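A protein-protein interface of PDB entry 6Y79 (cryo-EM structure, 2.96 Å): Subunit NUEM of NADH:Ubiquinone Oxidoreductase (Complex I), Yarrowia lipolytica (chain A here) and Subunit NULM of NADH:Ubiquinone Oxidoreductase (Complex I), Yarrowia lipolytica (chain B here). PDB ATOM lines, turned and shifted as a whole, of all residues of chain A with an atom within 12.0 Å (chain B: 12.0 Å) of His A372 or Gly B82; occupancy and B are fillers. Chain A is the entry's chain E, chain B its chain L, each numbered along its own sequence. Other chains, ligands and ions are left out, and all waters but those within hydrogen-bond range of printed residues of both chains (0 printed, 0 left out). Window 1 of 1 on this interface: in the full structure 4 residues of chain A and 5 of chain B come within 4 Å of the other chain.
The side-chain carboxylate of Glu A367 lies close to the backbone carbonyl oxygen of Gly B82.
The side-chain hydroxyl of Tyr B78 lies within hydrogen-bond range of the backbone carbonyl oxygen of Gly B82 (3.3 Å).
The side-chain amino group (NZ) of Lys A368 is in salt-bridge range of the side-chain carboxylate (OE1) of Glu A364 (3.9 Å).
OE1 of Glu A367 touches CB of Val B83 (3.7 Å).
Lys A368 touches Arg B81.
His A372 touches Gly B82 (CE1 to CA, 3.5 Å).
Tyr B78 touches Ile A373 (CD2 to CD1, 3.9 Å).
Ile A373 touches Arg B79.
Lys A366 touches none of the printed residues of chain B.
Glu A367 touches just these residues of chain B: Gly B82 and Val B83.
Of the printed residues of chain B, Lys A368 touches Arg B81 (3.7 Å).
No residue of chain B comes within 4 Å of Phe A370.
Val A371 touches none of the printed residues of chain B.
Of the printed residues of chain B, His A372 touches Gly B82.
Of the printed residues of chain B, Ile A373 touches Tyr B78 and Arg B79.
No residue of chain B comes within 4 Å of Leu A374.
Of the printed residues of chain A, Arg B79 touches Ile A373.
Printed residues of chain A within 4 Å of Arg B81: Lys A368.
Of the printed residues of chain A, Val B83 touches Glu A367 (3.7 Å).
The nearest residue of chain A that does not touch Gly B82 is Lys A368 (5.9 Å).
Along chain A the printed residues that touch a printed residue of chain B span positions 367 to 373.
Among the printed residues, no Asp or Glu carboxylate lies within 4 Å of a Lys or Arg side-chain nitrogen of the other chain.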
ATOM      1  N   VAL A 360     -28.845  -2.607  10.738  1.00  0.00           N
ATOM      2  CA  VAL A 360     -27.783  -3.232  11.515  1.00  0.00           C
ATOM      3  C   VAL A 360     -28.437  -4.295  12.397  1.00  0.00           C
ATOM      4  O   VAL A 360     -27.887  -5.387  12.591  1.00  0.00           O
ATOM      5  CB  VAL A 360     -26.992  -2.183  12.332  1.00  0.00           C
ATOM      6  CG1 VAL A 360     -25.894  -2.825  13.163  1.00  0.00           C
ATOM      7  CG2 VAL A 360     -26.401  -1.128  11.397  1.00  0.00           C
ATOM      8  N   GLN A 362     -31.824  -5.374  11.673  1.00  0.00           N
ATOM      9  CA  GLN A 362     -32.797  -6.173  10.921  1.00  0.00           C
ATOM     10  C   GLN A 362     -32.118  -6.999   9.831  1.00  0.00           C
ATOM     11  O   GLN A 362     -32.600  -8.095   9.497  1.00  0.00           O
ATOM     12  CB  GLN A 362     -33.923  -5.286  10.372  1.00  0.00           C
ATOM     13  CG  GLN A 362     -34.909  -4.905  11.494  1.00  0.00           C
ATOM     14  CD  GLN A 362     -34.475  -3.683  12.255  1.00  0.00           C
ATOM     15  OE1 GLN A 362     -33.652  -2.912  11.769  1.00  0.00           O
ATOM     16  NE2 GLN A 362     -35.018  -3.494  13.452  1.00  0.00           N
ATOM     17  N   LEU A 363     -30.948  -6.547   9.328  1.00  0.00           N
ATOM     18  CA  LEU A 363     -30.233  -7.366   8.358  1.00  0.00           C
ATOM     19  C   LEU A 363     -29.502  -8.523   9.043  1.00  0.00           C
ATOM     20  O   LEU A 363     -29.221  -9.523   8.383  1.00  0.00           O
ATOM     21  CB  LEU A 363     -29.291  -6.507   7.498  1.00  0.00           C
ATOM     22  CG  LEU A 363     -28.872  -7.230   6.198  1.00  0.00           C
ATOM     23  CD1 LEU A 363     -30.109  -7.785   5.449  1.00  0.00           C
ATOM     24  CD2 LEU A 363     -28.020  -6.404   5.218  1.00  0.00           C
ATOM     25  N   GLU A 364     -29.245  -8.456  10.374  1.00  0.00           N
ATOM     26  CA  GLU A 364     -28.708  -9.657  11.033  1.00  0.00           C
ATOM     27  C   GLU A 364     -29.723 -10.797  11.018  1.00  0.00           C
ATOM     28  O   GLU A 364     -29.371 -11.957  10.760  1.00  0.00           O
ATOM     29  CB  GLU A 364     -28.224  -9.395  12.463  1.00  0.00           C
ATOM     30  CG  GLU A 364     -29.226  -8.824  13.508  1.00  0.00           C
ATOM     31  CD  GLU A 364     -30.213  -9.847  14.139  1.00  0.00           C
ATOM     32  OE1 GLU A 364     -29.983 -11.076  14.136  1.00  0.00           O
ATOM     33  OE2 GLU A 364     -31.268  -9.381  14.623  1.00  0.00           O
ATOM     34  N   ASN A 365     -31.002 -10.484  11.229  1.00  0.00           N
ATOM     35  CA  ASN A 365     -31.993 -11.551  11.324  1.00  0.00           C
ATOM     36  C   ASN A 365     -32.479 -12.005   9.951  1.00  0.00           C
ATOM     37  O   ASN A 365     -32.971 -13.141   9.809  1.00  0.00           O
ATOM     38  CB  ASN A 365     -33.188 -11.140  12.183  1.00  0.00           C
ATOM     39  CG  ASN A 365     -33.970 -12.347  12.666  1.00  0.00           C
ATOM     40  OD1 ASN A 365     -33.527 -13.049  13.580  1.00  0.00           O
ATOM     41  ND2 ASN A 365     -35.096 -12.630  12.028  1.00  0.00           N
ATOM     42  N   LYS A 366     -32.400 -11.126   8.934  1.00  0.00           N
ATOM     43  CA  LYS A 366     -32.643 -11.626   7.584  1.00  0.00           C
ATOM     44  C   LYS A 366     -31.442 -12.412   7.077  1.00  0.00           C
ATOM     45  O   LYS A 366     -31.598 -13.336   6.262  1.00  0.00           O
ATOM     46  CB  LYS A 366     -32.995 -10.488   6.634  1.00  0.00           C
ATOM     47  CG  LYS A 366     -33.656 -11.001   5.320  1.00  0.00           C
ATOM     48  CD  LYS A 366     -34.396  -9.950   4.509  1.00  0.00           C
ATOM     49  CE  LYS A 366     -35.036 -10.596   3.284  1.00  0.00           C
ATOM     50  NZ  LYS A 366     -34.026 -10.901   2.233  1.00  0.00           N
ATOM     51  N   GLU A 367     -30.237 -12.072   7.574  1.00  0.00           N
ATOM     52  CA  GLU A 367     -29.047 -12.879   7.324  1.00  0.00           C
ATOM     53  C   GLU A 367     -29.171 -14.260   7.945  1.00  0.00           C
ATOM     54  O   GLU A 367     -28.618 -15.238   7.428  1.00  0.00           O
ATOM     55  CB  GLU A 367     -27.813 -12.193   7.887  1.00  0.00           C
ATOM     56  CG  GLU A 367     -27.018 -11.313   6.942  1.00  0.00           C
ATOM     57  CD  GLU A 367     -25.737 -10.804   7.575  1.00  0.00           C
ATOM     58  OE1 GLU A 367     -24.698 -11.462   7.401  1.00  0.00           O
ATOM     59  OE2 GLU A 367     -25.776  -9.777   8.289  1.00  0.00           O
ATOM     60  N   LYS A 368     -29.888 -14.357   9.059  1.00  0.00           N
ATOM     61  CA  LYS A 368     -30.135 -15.644   9.702  1.00  0.00           C
ATOM     62  C   LYS A 368     -30.940 -16.649   8.874  1.00  0.00           C
ATOM     63  O   LYS A 368     -31.108 -17.784   9.319  1.00  0.00           O
ATOM     64  CB  LYS A 368     -30.862 -15.436  11.030  1.00  0.00           C
ATOM     65  CG  LYS A 368     -30.009 -15.577  12.271  1.00  0.00           C
ATOM     66  CD  LYS A 368     -30.848 -15.200  13.491  1.00  0.00           C
ATOM     67  CE  LYS A 368     -30.094 -15.436  14.780  1.00  0.00           C
ATOM     68  NZ  LYS A 368     -28.792 -14.729  14.797  1.00  0.00           N
ATOM     69  N   THR A 369     -31.485 -16.267   7.711  1.00  0.00           N
ATOM     70  CA  THR A 369     -32.188 -17.214   6.853  1.00  0.00           C
ATOM     71  C   THR A 369     -31.447 -17.549   5.567  1.00  0.00           C
ATOM     72  O   THR A 369     -31.874 -18.458   4.850  1.00  0.00           O
ATOM     73  CB  THR A 369     -33.592 -16.699   6.494  1.00  0.00           C
ATOM     74  OG1 THR A 369     -33.494 -15.537   5.661  1.00  0.00           O
ATOM     75  CG2 THR A 369     -34.375 -16.361   7.748  1.00  0.00           C
ATOM     76  N   PHE A 370     -30.357 -16.853   5.259  1.00  0.00           N
ATOM     77  CA  PHE A 370     -29.558 -17.160   4.082  1.00  0.00           C
ATOM     78  C   PHE A 370     -28.524 -18.234   4.401  1.00  0.00           C
ATOM     79  O   PHE A 370     -28.385 -18.680   5.538  1.00  0.00           O
ATOM     80  CB  PHE A 370     -28.867 -15.905   3.549  1.00  0.00           C
ATOM     81  CG  PHE A 370     -29.811 -14.907   2.955  1.00  0.00           C
ATOM     82  CD1 PHE A 370     -30.445 -15.167   1.755  1.00  0.00           C
ATOM     83  CD2 PHE A 370     -30.059 -13.712   3.594  1.00  0.00           C
ATOM     84  CE1 PHE A 370     -31.324 -14.252   1.208  1.00  0.00           C
ATOM     85  CE2 PHE A 370     -30.939 -12.791   3.063  1.00  0.00           C
ATOM     86  CZ  PHE A 370     -31.567 -13.062   1.866  1.00  0.00           C
ATOM     87  N   VAL A 371     -27.797 -18.656   3.368  1.00  0.00           N
ATOM     88  CA  VAL A 371     -26.796 -19.709   3.464  1.00  0.00           C
ATOM     89  C   VAL A 371     -25.446 -19.101   3.125  1.00  0.00           C
ATOM     90  O   VAL A 371     -25.323 -18.383   2.128  1.00  0.00           O
ATOM     91  CB  VAL A 371     -27.125 -20.878   2.521  1.00  0.00           C
ATOM     92  CG1 VAL A 371     -26.110 -21.996   2.663  1.00  0.00           C
ATOM     93  CG2 VAL A 371     -28.502 -21.403   2.809  1.00  0.00           C
ATOM     94  N   HIS A 372     -24.431 -19.403   3.940  1.00  0.00           N
ATOM     95  CA  HIS A 372     -23.144 -18.736   3.834  1.00  0.00           C
ATOM     96  C   HIS A 372     -21.953 -19.655   3.580  1.00  0.00           C
ATOM     97  O   HIS A 372     -20.876 -19.146   3.255  1.00  0.00           O
ATOM     98  CB  HIS A 372     -22.875 -17.913   5.103  1.00  0.00           C
ATOM     99  CG  HIS A 372     -23.829 -16.775   5.294  1.00  0.00           C
ATOM    100  ND1 HIS A 372     -24.954 -16.867   6.085  1.00  0.00           N
ATOM    101  CD2 HIS A 372     -23.831 -15.520   4.785  1.00  0.00           C
ATOM    102  CE1 HIS A 372     -25.608 -15.721   6.051  1.00  0.00           C
ATOM    103  NE2 HIS A 372     -24.944 -14.885   5.277  1.00  0.00           N
ATOM    104  N   ILE A 373     -22.090 -20.975   3.753  1.00  0.00           N
ATOM    105  CA  ILE A 373     -20.984 -21.920   3.596  1.00  0.00           C
ATOM    106  C   ILE A 373     -21.313 -23.047   2.620  1.00  0.00           C
ATOM    107  O   ILE A 373     -20.449 -23.877   2.334  1.00  0.00           O
ATOM    108  CB  ILE A 373     -20.539 -22.496   4.970  1.00  0.00           C
ATOM    109  CG1 ILE A 373     -20.490 -21.418   6.047  1.00  0.00           C
ATOM    110  CG2 ILE A 373     -19.096 -23.091   5.001  1.00  0.00           C
ATOM    111  CD1 ILE A 373     -19.358 -20.419   5.946  1.00  0.00           C
ATOM    112  N   LEU A 374     -22.529 -23.088   2.065  1.00  0.00           N
ATOM    113  CA  LEU A 374     -23.007 -24.155   1.144  1.00  0.00           C
ATOM    114  C   LEU A 374     -22.909 -25.550   1.756  1.00  0.00           C
ATOM    115  O   LEU A 374     -21.953 -26.277   1.488  1.00  0.00           O
ATOM    116  CB  LEU A 374     -22.252 -24.168  -0.202  1.00  0.00           C
ATOM    117  CG  LEU A 374     -22.675 -23.361  -1.423  1.00  0.00           C
ATOM    118  CD1 LEU A 374     -24.061 -23.778  -1.887  1.00  0.00           C
ATOM    119  CD2 LEU A 374     -22.592 -21.889  -1.148  1.00  0.00           C
ATOM    120  N   ILE B  22     -13.149  -9.505  16.819  1.00  0.00           N
ATOM    121  CA  ILE B  22     -12.800 -10.799  17.369  1.00  0.00           C
ATOM    122  C   ILE B  22     -11.385 -11.229  16.996  1.00  0.00           C
ATOM    123  O   ILE B  22     -10.745 -11.938  17.777  1.00  0.00           O
ATOM    124  CB  ILE B  22     -13.840 -11.867  16.947  1.00  0.00           C
ATOM    125  CG1 ILE B  22     -13.712 -13.138  17.778  1.00  0.00           C
ATOM    126  CG2 ILE B  22     -13.751 -12.215  15.471  1.00  0.00           C
ATOM    127  CD1 ILE B  22     -13.919 -12.905  19.225  1.00  0.00           C
ATOM    128  N   LEU B  73     -13.146 -23.300  14.597  1.00  0.00           N
ATOM    129  CA  LEU B  73     -14.231 -22.966  15.521  1.00  0.00           C
ATOM    130  C   LEU B  73     -14.909 -21.650  15.148  1.00  0.00           C
ATOM    131  O   LEU B  73     -16.138 -21.538  15.224  1.00  0.00           O
ATOM    132  CB  LEU B  73     -13.706 -22.902  16.957  1.00  0.00           C
ATOM    133  CG  LEU B  73     -13.935 -24.019  17.972  1.00  0.00           C
ATOM    134  CD1 LEU B  73     -13.217 -25.273  17.602  1.00  0.00           C
ATOM    135  CD2 LEU B  73     -13.444 -23.540  19.299  1.00  0.00           C
ATOM    136  N   LEU B  74     -14.125 -20.646  14.729  1.00  0.00           N
ATOM    137  CA  LEU B  74     -14.708 -19.387  14.255  1.00  0.00           C
ATOM    138  C   LEU B  74     -15.492 -19.579  12.966  1.00  0.00           C
ATOM    139  O   LEU B  74     -16.517 -18.922  12.762  1.00  0.00           O
ATOM    140  CB  LEU B  74     -13.634 -18.317  14.055  1.00  0.00           C
ATOM    141  CG  LEU B  74     -14.082 -16.900  13.660  1.00  0.00           C
ATOM    142  CD1 LEU B  74     -13.258 -15.875  14.309  1.00  0.00           C
ATOM    143  CD2 LEU B  74     -13.944 -16.617  12.191  1.00  0.00           C
ATOM    144  N   VAL B  75     -15.011 -20.444  12.071  1.00  0.00           N
ATOM    145  CA  VAL B  75     -15.732 -20.685  10.822  1.00  0.00           C
ATOM    146  C   VAL B  75     -17.092 -21.317  11.101  1.00  0.00           C
ATOM    147  O   VAL B  75     -18.107 -20.917  10.518  1.00  0.00           O
ATOM    148  CB  VAL B  75     -14.876 -21.539   9.866  1.00  0.00           C
ATOM    149  CG1 VAL B  75     -15.681 -22.016   8.675  1.00  0.00           C
ATOM    150  CG2 VAL B  75     -13.696 -20.740   9.378  1.00  0.00           C
ATOM    151  N   SER B  76     -17.152 -22.256  12.051  1.00  0.00           N
ATOM    152  CA  SER B  76     -18.446 -22.836  12.415  1.00  0.00           C
ATOM    153  C   SER B  76     -19.322 -21.863  13.189  1.00  0.00           C
ATOM    154  O   SER B  76     -20.549 -21.995  13.182  1.00  0.00           O
ATOM    155  CB  SER B  76     -18.269 -24.095  13.235  1.00  0.00           C
ATOM    156  OG  SER B  76     -17.717 -23.828  14.505  1.00  0.00           O
ATOM    157  N   TYR B  77     -18.712 -20.921  13.915  1.00  0.00           N
ATOM    158  CA  TYR B  77     -19.487 -19.827  14.493  1.00  0.00           C
ATOM    159  C   TYR B  77     -20.131 -18.990  13.403  1.00  0.00           C
ATOM    160  O   TYR B  77     -21.267 -18.536  13.553  1.00  0.00           O
ATOM    161  CB  TYR B  77     -18.589 -18.957  15.369  1.00  0.00           C
ATOM    162  CG  TYR B  77     -19.289 -17.805  16.058  1.00  0.00           C
ATOM    163  CD1 TYR B  77     -19.913 -17.986  17.276  1.00  0.00           C
ATOM    164  CD2 TYR B  77     -19.301 -16.528  15.501  1.00  0.00           C
ATOM    165  CE1 TYR B  77     -20.546 -16.942  17.912  1.00  0.00           C
ATOM    166  CE2 TYR B  77     -19.939 -15.485  16.126  1.00  0.00           C
ATOM    167  CZ  TYR B  77     -20.559 -15.698  17.331  1.00  0.00           C
ATOM    168  OH  TYR B  77     -21.195 -14.660  17.961  1.00  0.00           O
ATOM    169  N   TYR B  78     -19.420 -18.795  12.301  1.00  0.00           N
ATOM    170  CA  TYR B  78     -19.857 -17.967  11.189  1.00  0.00           C
ATOM    171  C   TYR B  78     -20.841 -18.666  10.257  1.00  0.00           C
ATOM    172  O   TYR B  78     -21.527 -17.979   9.499  1.00  0.00           O
ATOM    173  CB  TYR B  78     -18.616 -17.516  10.411  1.00  0.00           C
ATOM    174  CG  TYR B  78     -18.854 -16.575   9.263  1.00  0.00           C
ATOM    175  CD1 TYR B  78     -18.979 -15.214   9.475  1.00  0.00           C
ATOM    176  CD2 TYR B  78     -18.931 -17.049   7.960  1.00  0.00           C
ATOM    177  CE1 TYR B  78     -19.191 -14.356   8.426  1.00  0.00           C
ATOM    178  CE2 TYR B  78     -19.150 -16.200   6.911  1.00  0.00           C
ATOM    179  CZ  TYR B  78     -19.274 -14.857   7.149  1.00  0.00           C
ATOM    180  OH  TYR B  78     -19.484 -14.008   6.096  1.00  0.00           O
ATOM    181  N   ARG B  79     -20.918 -20.004  10.288  1.00  0.00           N
ATOM    182  CA  ARG B  79     -21.800 -20.746   9.380  1.00  0.00           C
ATOM    183  C   ARG B  79     -23.261 -20.353   9.531  1.00  0.00           C
ATOM    184  O   ARG B  79     -23.963 -20.151   8.535  1.00  0.00           O
ATOM    185  CB  ARG B  79     -21.700 -22.247   9.621  1.00  0.00           C
ATOM    186  CG  ARG B  79     -20.395 -22.897   9.316  1.00  0.00           C
ATOM    187  CD  ARG B  79     -20.519 -24.384   9.538  1.00  0.00           C
ATOM    188  NE  ARG B  79     -21.502 -24.937   8.623  1.00  0.00           N
ATOM    189  CZ  ARG B  79     -21.187 -25.569   7.501  1.00  0.00           C
ATOM    190  NH1 ARG B  79     -22.140 -26.030   6.712  1.00  0.00           N
ATOM    191  NH2 ARG B  79     -19.915 -25.742   7.176  1.00  0.00           N
ATOM    192  N   LEU B  80     -23.739 -20.257  10.762  1.00  0.00           N
ATOM    193  CA  LEU B  80     -25.144 -19.999  11.016  1.00  0.00           C
ATOM    194  C   LEU B  80     -25.457 -18.523  11.140  1.00  0.00           C
ATOM    195  O   LEU B  80     -26.615 -18.128  10.987  1.00  0.00           O
ATOM    196  CB  LEU B  80     -25.570 -20.700  12.298  1.00  0.00           C
ATOM    197  CG  LEU B  80     -25.381 -22.200  12.410  1.00  0.00           C
ATOM    198  CD1 LEU B  80     -25.643 -22.550  13.826  1.00  0.00           C
ATOM    199  CD2 LEU B  80     -26.340 -22.929  11.503  1.00  0.00           C
ATOM    200  N   ARG B  81     -24.455 -17.711  11.427  1.00  0.00           N
ATOM    201  CA  ARG B  81     -24.593 -16.267  11.512  1.00  0.00           C
ATOM    202  C   ARG B  81     -23.610 -15.691  10.514  1.00  0.00           C
ATOM    203  O   ARG B  81     -22.413 -15.635  10.798  1.00  0.00           O
ATOM    204  CB  ARG B  81     -24.278 -15.764  12.920  1.00  0.00           C
ATOM    205  CG  ARG B  81     -25.422 -15.857  13.896  1.00  0.00           C
ATOM    206  CD  ARG B  81     -25.491 -17.222  14.549  1.00  0.00           C
ATOM    207  NE  ARG B  81     -24.406 -17.422  15.500  1.00  0.00           N
ATOM    208  CZ  ARG B  81     -23.960 -18.613  15.877  1.00  0.00           C
ATOM    209  NH1 ARG B  81     -24.480 -19.719  15.376  1.00  0.00           N
ATOM    210  NH2 ARG B  81     -22.985 -18.700  16.746  1.00  0.00           N
ATOM    211  N   GLY B  82     -24.098 -15.183   9.385  1.00  0.00           N
ATOM    212  CA  GLY B  82     -23.210 -14.708   8.332  1.00  0.00           C
ATOM    213  C   GLY B  82     -22.515 -13.384   8.595  1.00  0.00           C
ATOM    214  O   GLY B  82     -22.088 -12.687   7.671  1.00  0.00           O
ATOM    215  N   VAL B  83     -22.386 -13.051   9.872  1.00  0.00           N
ATOM    216  CA  VAL B  83     -21.852 -11.801  10.366  1.00  0.00           C
ATOM    217  C   VAL B  83     -21.098 -12.152  11.636  1.00  0.00           C
ATOM    218  O   VAL B  83     -21.412 -13.135  12.311  1.00  0.00           O
ATOM    219  CB  VAL B  83     -23.000 -10.781  10.603  1.00  0.00           C
ATOM    220  CG1 VAL B  83     -23.986 -11.273  11.666  1.00  0.00           C
ATOM    221  CG2 VAL B  83     -22.481  -9.404  10.957  1.00  0.00           C
ATOM    222  N   ILE B  84     -20.045 -11.405  11.920  1.00  0.00           N
ATOM    223  CA  ILE B  84     -19.397 -11.454  13.218  1.00  0.00           C
ATOM    224  C   ILE B  84     -19.507 -10.071  13.827  1.00  0.00           C
ATOM    225  O   ILE B  84     -19.128  -9.080  13.197  1.00  0.00           O
ATOM    226  CB  ILE B  84     -17.941 -11.923  13.115  1.00  0.00           C
ATOM    227  CG1 ILE B  84     -17.912 -13.360  12.606  1.00  0.00           C
ATOM    228  CG2 ILE B  84     -17.284 -11.860  14.464  1.00  0.00           C
ATOM    229  CD1 ILE B  84     -16.544 -13.885  12.382  1.00  0.00           C
ATOM    230  N   ASN B  85     -20.070 -10.007  15.027  1.00  0.00           N
ATOM    231  CA  ASN B  85     -20.348  -8.743  15.675  1.00  0.00           C
ATOM    232  C   ASN B  85     -19.060  -8.043  16.077  1.00  0.00           C
ATOM    233  O   ASN B  85     -18.012  -8.661  16.280  1.00  0.00           O
ATOM    234  CB  ASN B  85     -21.221  -8.960  16.903  1.00  0.00           C
ATOM    235  CG  ASN B  85     -22.586  -9.493  16.554  1.00  0.00           C
ATOM    236  OD1 ASN B  85     -23.195  -9.077  15.569  1.00  0.00           O
ATOM    237  ND2 ASN B  85     -23.082 -10.421  17.364  1.00  0.00           N
ATOM    238  N   SER B  86     -19.151  -6.723  16.182  1.00  0.00           N
ATOM    239  CA  SER B  86     -18.003  -5.947  16.617  1.00  0.00           C
ATOM    240  C   SER B  86     -17.808  -6.047  18.123  1.00  0.00           C
ATOM    241  O   SER B  86     -16.671  -6.118  18.599  1.00  0.00           O
ATOM    242  CB  SER B  86     -18.170  -4.493  16.193  1.00  0.00           C
ATOM    243  OG  SER B  86     -19.248  -3.885  16.880  1.00  0.00           O
ATOM    244  N   GLY B  88     -18.523  -8.515  20.116  1.00  0.00           N
ATOM    245  CA  GLY B  88     -17.979  -9.806  20.454  1.00  0.00           C
ATOM    246  C   GLY B  88     -18.965 -10.906  20.146  1.00  0.00           C
ATOM    247  O   GLY B  88     -19.998 -10.688  19.514  1.00  0.00           O
